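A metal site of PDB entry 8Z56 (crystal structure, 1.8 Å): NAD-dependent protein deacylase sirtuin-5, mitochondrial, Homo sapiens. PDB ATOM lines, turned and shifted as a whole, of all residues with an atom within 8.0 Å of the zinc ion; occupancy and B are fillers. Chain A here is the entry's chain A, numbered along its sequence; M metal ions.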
ATOM      1  N   ARG A 137     -11.328  11.034  19.582  1.00  0.00           N
ATOM      2  CA  ARG A 137     -10.910  11.222  18.211  1.00  0.00           C
ATOM      3  C   ARG A 137      -9.433  10.893  18.101  1.00  0.00           C
ATOM      4  O   ARG A 137      -8.633  11.299  18.956  1.00  0.00           O
ATOM      5  CB  ARG A 137     -11.159  12.665  17.733  1.00  0.00           C
ATOM      6  CG  ARG A 137     -10.932  12.802  16.255  1.00  0.00           C
ATOM      7  CD  ARG A 137     -11.503  14.113  15.724  1.00  0.00           C
ATOM      8  NE  ARG A 137     -10.616  15.242  15.953  1.00  0.00           N
ATOM      9  CZ  ARG A 137     -10.922  16.290  16.722  1.00  0.00           C
ATOM     10  NH1 ARG A 137     -12.095  16.355  17.347  1.00  0.00           N
ATOM     11  NH2 ARG A 137     -10.064  17.298  16.847  1.00  0.00           N
ATOM     12  N   CYS A 138      -9.070  10.183  17.048  1.00  0.00           N
ATOM     13  CA  CYS A 138      -7.686   9.735  16.904  1.00  0.00           C
ATOM     14  C   CYS A 138      -6.828  10.831  16.280  1.00  0.00           C
ATOM     15  O   CYS A 138      -7.152  11.350  15.204  1.00  0.00           O
ATOM     16  CB  CYS A 138      -7.595   8.473  16.049  1.00  0.00           C
ATOM     17  SG  CYS A 138      -5.870   8.002  15.778  1.00  0.00           S
ATOM     18  N   THR A 139      -5.736  11.186  16.953  1.00  0.00           N
ATOM     19  CA  THR A 139      -4.876  12.230  16.414  1.00  0.00           C
ATOM     20  C   THR A 139      -4.117  11.795  15.166  1.00  0.00           C
ATOM     21  O   THR A 139      -3.424  12.616  14.572  1.00  0.00           O
ATOM     22  CB  THR A 139      -3.887  12.758  17.455  1.00  0.00           C
ATOM     23  OG1 THR A 139      -3.065  11.688  17.959  1.00  0.00           O
ATOM     24  CG2 THR A 139      -4.631  13.449  18.606  1.00  0.00           C
ATOM     25  N   SER A 140      -4.240  10.536  14.738  1.00  0.00           N
ATOM     26  CA  SER A 140      -3.557  10.057  13.549  1.00  0.00           C
ATOM     27  C   SER A 140      -4.507   9.793  12.393  1.00  0.00           C
ATOM     28  O   SER A 140      -4.311  10.339  11.296  1.00  0.00           O
ATOM     29  CB  SER A 140      -2.719   8.804  13.847  1.00  0.00           C
ATOM     30  OG  SER A 140      -1.716   9.068  14.815  1.00  0.00           O
ATOM     31  N   CYS A 141      -5.547   8.986  12.604  1.00  0.00           N
ATOM     32  CA  CYS A 141      -6.444   8.608  11.515  1.00  0.00           C
ATOM     33  C   CYS A 141      -7.753   9.389  11.514  1.00  0.00           C
ATOM     34  O   CYS A 141      -8.470   9.346  10.510  1.00  0.00           O
ATOM     35  CB  CYS A 141      -6.736   7.097  11.549  1.00  0.00           C
ATOM     36  SG  CYS A 141      -7.744   6.543  12.930  1.00  0.00           S
ATOM     37  N   GLY A 142      -8.070  10.099  12.597  1.00  0.00           N
ATOM     38  CA  GLY A 142      -9.232  10.980  12.623  1.00  0.00           C
ATOM     39  C   GLY A 142     -10.555  10.323  12.954  1.00  0.00           C
ATOM     40  O   GLY A 142     -11.584  11.021  12.985  1.00  0.00           O
ATOM     41  N   VAL A 143     -10.571   9.012  13.215  1.00  0.00           N
ATOM     42  CA  VAL A 143     -11.826   8.334  13.523  1.00  0.00           C
ATOM     43  C   VAL A 143     -12.370   8.800  14.867  1.00  0.00           C
ATOM     44  O   VAL A 143     -11.616   9.038  15.814  1.00  0.00           O
ATOM     45  CB  VAL A 143     -11.661   6.806  13.462  1.00  0.00           C
ATOM     46  CG1 VAL A 143     -10.791   6.326  14.603  1.00  0.00           C
ATOM     47  CG2 VAL A 143     -13.019   6.123  13.531  1.00  0.00           C
ATOM     48  N   VAL A 144     -13.696   8.955  14.932  1.00  0.00           N
ATOM     49  CA  VAL A 144     -14.405   9.399  16.114  1.00  0.00           C
ATOM     50  C   VAL A 144     -15.226   8.220  16.638  1.00  0.00           C
ATOM     51  O   VAL A 144     -15.880   7.524  15.856  1.00  0.00           O
ATOM     52  CB  VAL A 144     -15.329  10.583  15.773  1.00  0.00           C
ATOM     53  CG1 VAL A 144     -16.123  11.016  16.982  1.00  0.00           C
ATOM     54  CG2 VAL A 144     -14.507  11.757  15.186  1.00  0.00           C
ATOM     55  N   ARG A 178      -5.456   4.770  23.242  1.00  0.00           N
ATOM     56  CA  ARG A 178      -4.881   4.520  21.928  1.00  0.00           C
ATOM     57  C   ARG A 178      -5.974   4.047  20.979  1.00  0.00           C
ATOM     58  O   ARG A 178      -6.913   3.344  21.374  1.00  0.00           O
ATOM     59  CB  ARG A 178      -3.762   3.464  22.048  1.00  0.00           C
ATOM     60  CG  ARG A 178      -2.607   3.735  21.156  1.00  0.00           C
ATOM     61  CD  ARG A 178      -1.862   4.999  21.525  1.00  0.00           C
ATOM     62  NE  ARG A 178      -0.924   5.357  20.467  1.00  0.00           N
ATOM     63  CZ  ARG A 178       0.007   6.294  20.571  1.00  0.00           C
ATOM     64  NH1 ARG A 178       0.135   6.980  21.703  1.00  0.00           N
ATOM     65  NH2 ARG A 178       0.819   6.538  19.556  1.00  0.00           N
ATOM     66  N   CYS A 179      -5.829   4.422  19.702  1.00  0.00           N
ATOM     67  CA  CYS A 179      -6.799   4.055  18.680  1.00  0.00           C
ATOM     68  C   CYS A 179      -6.775   2.559  18.459  1.00  0.00           C
ATOM     69  O   CYS A 179      -5.703   1.958  18.342  1.00  0.00           O
ATOM     70  CB  CYS A 179      -6.456   4.769  17.375  1.00  0.00           C
ATOM     71  SG  CYS A 179      -7.635   4.452  16.030  1.00  0.00           S
ATOM     72  N   GLU A 180      -7.957   1.943  18.401  1.00  0.00           N
ATOM     73  CA  GLU A 180      -8.058   0.512  18.152  1.00  0.00           C
ATOM     74  C   GLU A 180      -8.457   0.205  16.715  1.00  0.00           C
ATOM     75  O   GLU A 180      -8.776  -0.949  16.403  1.00  0.00           O
ATOM     76  CB  GLU A 180      -8.998  -0.161  19.145  1.00  0.00           C
ATOM     77  CG  GLU A 180      -8.760   0.298  20.579  1.00  0.00           C
ATOM     78  CD  GLU A 180      -9.314  -0.656  21.605  1.00  0.00           C
ATOM     79  OE1 GLU A 180      -8.558  -1.536  22.064  1.00  0.00           O
ATOM     80  OE2 GLU A 180     -10.501  -0.532  21.964  1.00  0.00           O
ATOM     81  N   GLU A 181      -8.443   1.202  15.836  1.00  0.00           N
ATOM     82  CA  GLU A 181      -8.561   0.919  14.406  1.00  0.00           C
ATOM     83  C   GLU A 181      -7.366   0.076  13.971  1.00  0.00           C
ATOM     84  O   GLU A 181      -6.213   0.443  14.204  1.00  0.00           O
ATOM     85  CB  GLU A 181      -8.591   2.235  13.624  1.00  0.00           C
ATOM     86  CG  GLU A 181      -9.772   2.396  12.682  1.00  0.00           C
ATOM     87  CD  GLU A 181     -11.106   2.195  13.367  1.00  0.00           C
ATOM     88  OE1 GLU A 181     -12.052   1.721  12.708  1.00  0.00           O
ATOM     89  OE2 GLU A 181     -11.211   2.517  14.568  1.00  0.00           O
ATOM     90  N   ALA A 182      -7.658  -1.073  13.371  1.00  0.00           N
ATOM     91  CA  ALA A 182      -6.602  -1.982  12.966  1.00  0.00           C
ATOM     92  C   ALA A 182      -5.592  -1.248  12.119  1.00  0.00           C
ATOM     93  O   ALA A 182      -5.948  -0.509  11.195  1.00  0.00           O
ATOM     94  CB  ALA A 182      -7.200  -3.148  12.186  1.00  0.00           C
ATOM     95  N   GLY A 183      -4.324  -1.410  12.473  1.00  0.00           N
ATOM     96  CA  GLY A 183      -3.231  -0.742  11.792  1.00  0.00           C
ATOM     97  C   GLY A 183      -2.873   0.633  12.323  1.00  0.00           C
ATOM     98  O   GLY A 183      -1.788   1.119  12.005  1.00  0.00           O
ATOM     99  N   CYS A 184      -3.734   1.268  13.109  1.00  0.00           N
ATOM    100  CA  CYS A 184      -3.447   2.665  13.496  1.00  0.00           C
ATOM    101  C   CYS A 184      -2.758   2.782  14.864  1.00  0.00           C
ATOM    102  O   CYS A 184      -1.586   3.114  14.942  1.00  0.00           O
ATOM    103  CB  CYS A 184      -4.727   3.493  13.469  1.00  0.00           C
ATOM    104  SG  CYS A 184      -4.369   5.151  13.977  1.00  0.00           S
ATOM    105  N   GLY A 185      -3.487   2.455  15.934  1.00  0.00           N
ATOM    106  CA  GLY A 185      -2.956   2.647  17.276  1.00  0.00           C
ATOM    107  C   GLY A 185      -2.417   4.030  17.569  1.00  0.00           C
ATOM    108  O   GLY A 185      -1.522   4.172  18.408  1.00  0.00           O
ATOM    109  N   GLY A 186      -2.929   5.052  16.885  1.00  0.00           N
ATOM    110  CA  GLY A 186      -2.507   6.404  17.172  1.00  0.00           C
ATOM    111  C   GLY A 186      -3.080   6.901  18.483  1.00  0.00           C
ATOM    112  O   GLY A 186      -3.975   6.311  19.080  1.00  0.00           O
ATOM    113  N   LEU A 187      -2.538   8.018  18.951  1.00  0.00           N
ATOM    114  CA  LEU A 187      -2.990   8.595  20.215  1.00  0.00           C
ATOM    115  C   LEU A 187      -4.383   9.203  20.039  1.00  0.00           C
ATOM    116  O   LEU A 187      -4.654   9.906  19.067  1.00  0.00           O
ATOM    117  CB  LEU A 187      -2.002   9.664  20.675  1.00  0.00           C
ATOM    118  CG  LEU A 187      -2.407  10.467  21.918  1.00  0.00           C
ATOM    119  CD1 LEU A 187      -2.457   9.599  23.168  1.00  0.00           C
ATOM    120  CD2 LEU A 187      -1.485  11.666  22.128  1.00  0.00           C
ATOM    121  N   LEU A 188      -5.265   8.940  21.003  1.00  0.00           N
ATOM    122  CA  LEU A 188      -6.588   9.558  21.015  1.00  0.00           C
ATOM    123  C   LEU A 188      -6.548  10.863  21.792  1.00  0.00           C
ATOM    124  O   LEU A 188      -5.753  11.038  22.720  1.00  0.00           O
ATOM    125  CB  LEU A 188      -7.596   8.617  21.691  1.00  0.00           C
ATOM    126  CG  LEU A 188      -7.744   7.219  21.080  1.00  0.00           C
ATOM    127  CD1 LEU A 188      -8.828   6.428  21.801  1.00  0.00           C
ATOM    128  CD2 LEU A 188      -8.074   7.322  19.606  1.00  0.00           C
HETATM  129 ZN    ZN M   1      -6.305   6.088  14.749  1.00  0.00          ZN
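O of Val 143 sits at hydrogen-bond distance from N of Cys 138, 3.1 Å away. SG of Cys 138 sits close to N of Ser 140. SG of Cys 184 lies close to N of Gly 186 (3.2 Å). The backbone NH (N) of Val 143 sits close to the side-chain sulfur (SG) of Cys 141 (3.8 Å). N of Cys 179 sits at hydrogen-bond distance from O of Gly 186, at 2.7 Å. The side-chain sulfur (SG) of Cys 179 sits close to the backbone NH (N) of Glu 181 (3.4 Å). N of Gly 185 lies close to O of Cys 179.
Four residues have an atom within 4 Å of the zinc ion: Cys 138, Cys 141, Cys 179 and Cys 184. The nearest printed residue that does not touch the zinc ion is Gly 186 (4.1 Å).
The zinc ion is bound by SG of Cys 138, SG of Cys 184, SG of Cys 141 and SG of Cys 179. The zinc ion has four donor atoms within binding distance.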
